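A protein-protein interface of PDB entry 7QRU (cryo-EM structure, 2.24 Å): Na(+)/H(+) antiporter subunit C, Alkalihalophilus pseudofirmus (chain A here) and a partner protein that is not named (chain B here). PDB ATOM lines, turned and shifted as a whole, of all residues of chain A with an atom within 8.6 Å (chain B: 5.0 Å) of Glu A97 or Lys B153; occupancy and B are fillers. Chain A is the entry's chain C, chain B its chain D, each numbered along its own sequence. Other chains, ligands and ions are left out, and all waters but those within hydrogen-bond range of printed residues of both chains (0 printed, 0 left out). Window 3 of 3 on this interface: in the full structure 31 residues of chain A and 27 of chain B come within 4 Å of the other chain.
The backbone carbonyl oxygen of Thr A94 is in hydrogen-bond range of a ring nitrogen (ND1) of His A98. OG1 of Thr A94 lies within hydrogen-bond range of O of Leu A90, at 2.8 Å. NH2 of Arg A93 is in salt-bridge range of OE1 of Glu A97 (3.3 Å).
Glu A97 touches just these residues of chain B: Lys B153 and Leu B156. Of chain A, only Glu A97 (3.8 Å) and His A98 (3.1 Å) come within 4 Å of Lys B153. Of the printed residues of chain B, His A98 touches Lys B153 (3.1 Å) and Arg B157 (3.8 Å). Of the printed residues of chain A, Leu B156 touches Leu A90, Arg A93, Thr A94 and Glu A97. Printed residues of chain A within 4 Å of Arg B157: His A98 and Leu A106. Tyr B154 touches none of the printed residues of chain A. Tyr A92 touches none of the printed residues of chain B. The nearest residue of chain B that does not touch Glu A97 is Gly B151 (4.9 Å). The nearest residue of chain A that does not touch Lys B153 is Thr A94 (6.1 Å). The nearest printed residue of chain A that does not touch Leu B156 is His A98 (4.2 Å).
Among the printed residues, merely in contact across the chains: Leu A106 with Arg B157 (3.6 Å), Glu A97 with Leu B156 (3.6 Å), Thr A94 with Leu B156 (3.6 Å), Arg A93 with Leu B156 (3.7 Å), Glu A97 with Lys B153 (3.8 Å), His A98 with Arg B157 (3.8 Å) and Leu A90 with Leu B156 (3.9 Å).
The backbone carbonyl oxygen (O) of Lys B153 sits close to a ring nitrogen (NE2) of His A98 (3.1 Å).
Of the 7 printed residues of chain B, 3 touch a printed residue of chain A. Printed residues of chain B that touch a printed residue of chain A: Lys B153, Leu B156 and Arg B157. Among the printed residues, 8 pairs touch across the chains.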
ATOM      1  N   LEU A  90      20.279 -25.485  14.540  1.00  0.00           N
ATOM      2  CA  LEU A  90      19.906 -25.052  15.861  1.00  0.00           C
ATOM      3  C   LEU A  90      19.710 -26.253  16.785  1.00  0.00           C
ATOM      4  O   LEU A  90      20.197 -26.230  17.900  1.00  0.00           O
ATOM      5  CB  LEU A  90      18.635 -24.230  15.729  1.00  0.00           C
ATOM      6  CG  LEU A  90      18.013 -23.722  17.029  1.00  0.00           C
ATOM      7  CD1 LEU A  90      19.044 -22.982  17.849  1.00  0.00           C
ATOM      8  CD2 LEU A  90      16.841 -22.827  16.709  1.00  0.00           C
ATOM      9  N   ALA A  91      19.133 -27.340  16.292  1.00  0.00           N
ATOM     10  CA  ALA A  91      18.945 -28.555  17.079  1.00  0.00           C
ATOM     11  C   ALA A  91      20.250 -29.135  17.551  1.00  0.00           C
ATOM     12  O   ALA A  91      20.400 -29.388  18.739  1.00  0.00           O
ATOM     13  CB  ALA A  91      18.230 -29.559  16.301  1.00  0.00           C
ATOM     14  N   TYR A  92      21.227 -29.275  16.674  1.00  0.00           N
ATOM     15  CA  TYR A  92      22.478 -29.883  17.119  1.00  0.00           C
ATOM     16  C   TYR A  92      23.267 -28.941  18.039  1.00  0.00           C
ATOM     17  O   TYR A  92      23.818 -29.357  19.028  1.00  0.00           O
ATOM     18  CB  TYR A  92      23.267 -30.439  15.912  1.00  0.00           C
ATOM     19  CG  TYR A  92      24.340 -29.592  15.295  1.00  0.00           C
ATOM     20  CD1 TYR A  92      25.462 -29.244  16.031  1.00  0.00           C
ATOM     21  CD2 TYR A  92      24.301 -29.274  13.964  1.00  0.00           C
ATOM     22  CE1 TYR A  92      26.514 -28.533  15.454  1.00  0.00           C
ATOM     23  CE2 TYR A  92      25.345 -28.584  13.362  1.00  0.00           C
ATOM     24  CZ  TYR A  92      26.478 -28.263  14.111  1.00  0.00           C
ATOM     25  OH  TYR A  92      27.560 -27.527  13.726  1.00  0.00           O
ATOM     26  N   ARG A  93      23.271 -27.648  17.786  1.00  0.00           N
ATOM     27  CA  ARG A  93      23.937 -26.715  18.698  1.00  0.00           C
ATOM     28  C   ARG A  93      23.287 -26.807  20.076  1.00  0.00           C
ATOM     29  O   ARG A  93      23.960 -26.717  21.037  1.00  0.00           O
ATOM     30  CB  ARG A  93      23.857 -25.280  18.165  1.00  0.00           C
ATOM     31  CG  ARG A  93      24.841 -24.967  17.048  1.00  0.00           C
ATOM     32  CD  ARG A  93      26.275 -24.854  17.452  1.00  0.00           C
ATOM     33  NE  ARG A  93      26.434 -24.530  18.886  1.00  0.00           N
ATOM     34  CZ  ARG A  93      26.612 -23.302  19.329  1.00  0.00           C
ATOM     35  NH1 ARG A  93      26.539 -22.259  18.530  1.00  0.00           N
ATOM     36  NH2 ARG A  93      26.832 -23.066  20.595  1.00  0.00           N
ATOM     37  N   THR A  94      21.950 -26.981  20.153  1.00  0.00           N
ATOM     38  CA  THR A  94      21.237 -27.147  21.411  1.00  0.00           C
ATOM     39  C   THR A  94      21.639 -28.454  22.107  1.00  0.00           C
ATOM     40  O   THR A  94      21.804 -28.479  23.302  1.00  0.00           O
ATOM     41  CB  THR A  94      19.718 -27.116  21.227  1.00  0.00           C
ATOM     42  OG1 THR A  94      19.449 -25.886  20.601  1.00  0.00           O
ATOM     43  CG2 THR A  94      18.925 -27.259  22.509  1.00  0.00           C
ATOM     44  N   TYR A  95      21.810 -29.529  21.378  1.00  0.00           N
ATOM     45  CA  TYR A  95      22.136 -30.801  21.975  1.00  0.00           C
ATOM     46  C   TYR A  95      23.523 -30.677  22.564  1.00  0.00           C
ATOM     47  O   TYR A  95      23.739 -31.184  23.656  1.00  0.00           O
ATOM     48  CB  TYR A  95      22.161 -31.954  20.933  1.00  0.00           C
ATOM     49  CG  TYR A  95      22.839 -33.205  21.438  1.00  0.00           C
ATOM     50  CD1 TYR A  95      22.263 -34.016  22.431  1.00  0.00           C
ATOM     51  CD2 TYR A  95      24.113 -33.545  20.996  1.00  0.00           C
ATOM     52  CE1 TYR A  95      22.937 -35.114  22.956  1.00  0.00           C
ATOM     53  CE2 TYR A  95      24.752 -34.685  21.467  1.00  0.00           C
ATOM     54  CZ  TYR A  95      24.154 -35.484  22.428  1.00  0.00           C
ATOM     55  OH  TYR A  95      24.803 -36.591  22.924  1.00  0.00           O
ATOM     56  N   LYS A  96      24.457 -30.037  21.818  1.00  0.00           N
ATOM     57  CA  LYS A  96      25.859 -30.011  22.201  1.00  0.00           C
ATOM     58  C   LYS A  96      26.005 -29.260  23.505  1.00  0.00           C
ATOM     59  O   LYS A  96      26.736 -29.658  24.379  1.00  0.00           O
ATOM     60  CB  LYS A  96      26.725 -29.454  21.106  1.00  0.00           C
ATOM     61  CG  LYS A  96      26.998 -30.510  20.039  1.00  0.00           C
ATOM     62  CD  LYS A  96      28.399 -31.026  20.042  1.00  0.00           C
ATOM     63  CE  LYS A  96      28.528 -32.418  19.470  1.00  0.00           C
ATOM     64  NZ  LYS A  96      27.910 -33.441  20.372  1.00  0.00           N
ATOM     65  N   GLU A  97      25.233 -28.181  23.664  1.00  0.00           N
ATOM     66  CA  GLU A  97      25.371 -27.321  24.800  1.00  0.00           C
ATOM     67  C   GLU A  97      24.717 -27.961  26.003  1.00  0.00           C
ATOM     68  O   GLU A  97      25.211 -27.773  27.090  1.00  0.00           O
ATOM     69  CB  GLU A  97      24.918 -25.920  24.407  1.00  0.00           C
ATOM     70  CG  GLU A  97      25.947 -25.255  23.506  1.00  0.00           C
ATOM     71  CD  GLU A  97      27.195 -24.666  24.153  1.00  0.00           C
ATOM     72  OE1 GLU A  97      28.112 -24.304  23.375  1.00  0.00           O
ATOM     73  OE2 GLU A  97      27.237 -24.539  25.405  1.00  0.00           O
ATOM     74  N   HIS A  98      23.578 -28.588  25.843  1.00  0.00           N
ATOM     75  CA  HIS A  98      22.802 -29.161  26.956  1.00  0.00           C
ATOM     76  C   HIS A  98      23.119 -30.629  27.193  1.00  0.00           C
ATOM     77  O   HIS A  98      22.693 -31.168  28.204  1.00  0.00           O
ATOM     78  CB  HIS A  98      21.281 -29.002  26.748  1.00  0.00           C
ATOM     79  CG  HIS A  98      20.895 -27.561  26.720  1.00  0.00           C
ATOM     80  ND1 HIS A  98      20.961 -26.807  25.590  1.00  0.00           N
ATOM     81  CD2 HIS A  98      20.502 -26.749  27.727  1.00  0.00           C
ATOM     82  CE1 HIS A  98      20.606 -25.582  25.887  1.00  0.00           C
ATOM     83  NE2 HIS A  98      20.340 -25.497  27.206  1.00  0.00           N
ATOM     84  N   LYS A  99      23.837 -31.246  26.278  1.00  0.00           N
ATOM     85  CA  LYS A  99      24.169 -32.667  26.382  1.00  0.00           C
ATOM     86  C   LYS A  99      22.926 -33.540  26.489  1.00  0.00           C
ATOM     87  O   LYS A  99      23.026 -34.689  26.944  1.00  0.00           O
ATOM     88  CB  LYS A  99      25.151 -32.837  27.553  1.00  0.00           C
ATOM     89  CG  LYS A  99      26.499 -32.181  27.264  1.00  0.00           C
ATOM     90  CD  LYS A  99      27.409 -31.966  28.442  1.00  0.00           C
ATOM     91  CE  LYS A  99      28.598 -31.106  28.069  1.00  0.00           C
ATOM     92  NZ  LYS A  99      29.357 -31.678  26.929  1.00  0.00           N
ATOM     93  N   THR A 100      21.788 -33.071  25.973  1.00  0.00           N
ATOM     94  CA  THR A 100      20.568 -33.895  25.917  1.00  0.00           C
ATOM     95  C   THR A 100      19.757 -33.593  24.685  1.00  0.00           C
ATOM     96  O   THR A 100      19.791 -32.454  24.228  1.00  0.00           O
ATOM     97  CB  THR A 100      19.712 -33.686  27.184  1.00  0.00           C
ATOM     98  OG1 THR A 100      18.551 -34.492  27.034  1.00  0.00           O
ATOM     99  CG2 THR A 100      19.330 -32.247  27.471  1.00  0.00           C
ATOM    100  N   GLN A 105      14.154 -32.718  29.286  1.00  0.00           N
ATOM    101  CA  GLN A 105      15.303 -32.177  29.972  1.00  0.00           C
ATOM    102  C   GLN A 105      15.553 -30.740  29.569  1.00  0.00           C
ATOM    103  O   GLN A 105      16.383 -30.088  30.185  1.00  0.00           O
ATOM    104  CB  GLN A 105      16.570 -32.969  29.665  1.00  0.00           C
ATOM    105  CG  GLN A 105      16.416 -34.491  29.800  1.00  0.00           C
ATOM    106  CD  GLN A 105      16.034 -34.884  31.188  1.00  0.00           C
ATOM    107  OE1 GLN A 105      16.585 -34.360  32.156  1.00  0.00           O
ATOM    108  NE2 GLN A 105      15.107 -35.832  31.294  1.00  0.00           N
ATOM    109  N   LEU A 106      14.879 -30.260  28.523  1.00  0.00           N
ATOM    110  CA  LEU A 106      15.079 -28.887  28.053  1.00  0.00           C
ATOM    111  C   LEU A 106      13.991 -27.975  28.602  1.00  0.00           C
ATOM    112  O   LEU A 106      13.716 -26.936  28.030  1.00  0.00           O
ATOM    113  CB  LEU A 106      15.103 -28.880  26.514  1.00  0.00           C
ATOM    114  CG  LEU A 106      16.279 -29.664  25.948  1.00  0.00           C
ATOM    115  CD1 LEU A 106      16.225 -29.783  24.451  1.00  0.00           C
ATOM    116  CD2 LEU A 106      17.561 -29.045  26.339  1.00  0.00           C
ATOM    117  N   GLY B 151      24.140 -17.673  20.945  1.00  0.00           N
ATOM    118  CA  GLY B 151      23.996 -19.051  21.439  1.00  0.00           C
ATOM    119  C   GLY B 151      24.455 -19.385  22.881  1.00  0.00           C
ATOM    120  O   GLY B 151      25.242 -20.313  23.066  1.00  0.00           O
ATOM    121  N   THR B 152      24.012 -18.601  23.864  1.00  0.00           N
ATOM    122  CA  THR B 152      23.958 -18.990  25.268  1.00  0.00           C
ATOM    123  C   THR B 152      23.029 -20.191  25.443  1.00  0.00           C
ATOM    124  O   THR B 152      22.161 -20.419  24.598  1.00  0.00           O
ATOM    125  CB  THR B 152      23.470 -17.822  26.142  1.00  0.00           C
ATOM    126  OG1 THR B 152      22.120 -17.542  25.805  1.00  0.00           O
ATOM    127  CG2 THR B 152      24.244 -16.524  25.947  1.00  0.00           C
ATOM    128  N   LYS B 153      23.153 -20.938  26.542  1.00  0.00           N
ATOM    129  CA  LYS B 153      22.343 -22.146  26.703  1.00  0.00           C
ATOM    130  C   LYS B 153      20.892 -21.794  26.783  1.00  0.00           C
ATOM    131  O   LYS B 153      20.106 -22.560  26.224  1.00  0.00           O
ATOM    132  CB  LYS B 153      22.655 -22.953  27.964  1.00  0.00           C
ATOM    133  CG  LYS B 153      24.000 -23.633  27.839  1.00  0.00           C
ATOM    134  CD  LYS B 153      24.353 -24.548  28.978  1.00  0.00           C
ATOM    135  CE  LYS B 153      23.168 -25.173  29.658  1.00  0.00           C
ATOM    136  NZ  LYS B 153      23.625 -26.231  30.594  1.00  0.00           N
ATOM    137  N   TYR B 154      20.545 -20.667  27.498  1.00  0.00           N
ATOM    138  CA  TYR B 154      19.150 -20.333  27.530  1.00  0.00           C
ATOM    139  C   TYR B 154      18.693 -20.089  26.098  1.00  0.00           C
ATOM    140  O   TYR B 154      17.610 -20.490  25.729  1.00  0.00           O
ATOM    141  CB  TYR B 154      18.968 -19.155  28.460  1.00  0.00           C
ATOM    142  CG  TYR B 154      17.560 -18.696  28.629  1.00  0.00           C
ATOM    143  CD1 TYR B 154      16.971 -17.803  27.716  1.00  0.00           C
ATOM    144  CD2 TYR B 154      16.773 -19.203  29.639  1.00  0.00           C
ATOM    145  CE1 TYR B 154      15.630 -17.435  27.812  1.00  0.00           C
ATOM    146  CE2 TYR B 154      15.448 -18.767  29.784  1.00  0.00           C
ATOM    147  CZ  TYR B 154      14.853 -17.917  28.872  1.00  0.00           C
ATOM    148  OH  TYR B 154      13.476 -17.617  28.969  1.00  0.00           O
ATOM    149  N   GLN B 155      19.444 -19.266  25.360  1.00  0.00           N
ATOM    150  CA  GLN B 155      18.996 -18.834  24.065  1.00  0.00           C
ATOM    151  C   GLN B 155      18.779 -20.049  23.216  1.00  0.00           C
ATOM    152  O   GLN B 155      17.738 -20.096  22.541  1.00  0.00           O
ATOM    153  CB  GLN B 155      19.926 -17.903  23.303  1.00  0.00           C
ATOM    154  CG  GLN B 155      19.669 -16.458  23.654  1.00  0.00           C
ATOM    155  CD  GLN B 155      20.612 -15.574  22.871  1.00  0.00           C
ATOM    156  OE1 GLN B 155      21.799 -15.587  23.181  1.00  0.00           O
ATOM    157  NE2 GLN B 155      20.055 -14.757  21.942  1.00  0.00           N
ATOM    158  N   LEU B 156      19.630 -21.051  23.302  1.00  0.00           N
ATOM    159  CA  LEU B 156      19.476 -22.206  22.422  1.00  0.00           C
ATOM    160  C   LEU B 156      18.230 -22.990  22.822  1.00  0.00           C
ATOM    161  O   LEU B 156      17.383 -23.169  21.973  1.00  0.00           O
ATOM    162  CB  LEU B 156      20.707 -23.081  22.554  1.00  0.00           C
ATOM    163  CG  LEU B 156      21.981 -22.485  21.931  1.00  0.00           C
ATOM    164  CD1 LEU B 156      23.159 -23.306  22.274  1.00  0.00           C
ATOM    165  CD2 LEU B 156      21.871 -22.365  20.434  1.00  0.00           C
ATOM    166  N   ARG B 157      18.020 -23.337  24.092  1.00  0.00           N
ATOM    167  CA  ARG B 157      16.817 -24.081  24.400  1.00  0.00           C
ATOM    168  C   ARG B 157      15.479 -23.323  24.115  1.00  0.00           C
ATOM    169  O   ARG B 157      14.523 -23.897  23.703  1.00  0.00           O
ATOM    170  CB  ARG B 157      16.852 -24.694  25.800  1.00  0.00           C
ATOM    171  CG  ARG B 157      16.907 -23.747  26.944  1.00  0.00           C
ATOM    172  CD  ARG B 157      16.340 -24.527  28.182  1.00  0.00           C
ATOM    173  NE  ARG B 157      16.875 -23.862  29.399  1.00  0.00           N
ATOM    174  CZ  ARG B 157      16.241 -22.855  30.025  1.00  0.00           C
ATOM    175  NH1 ARG B 157      15.003 -22.580  29.681  1.00  0.00           N
ATOM    176  NH2 ARG B 157      16.809 -22.199  31.014  1.00  0.00           N
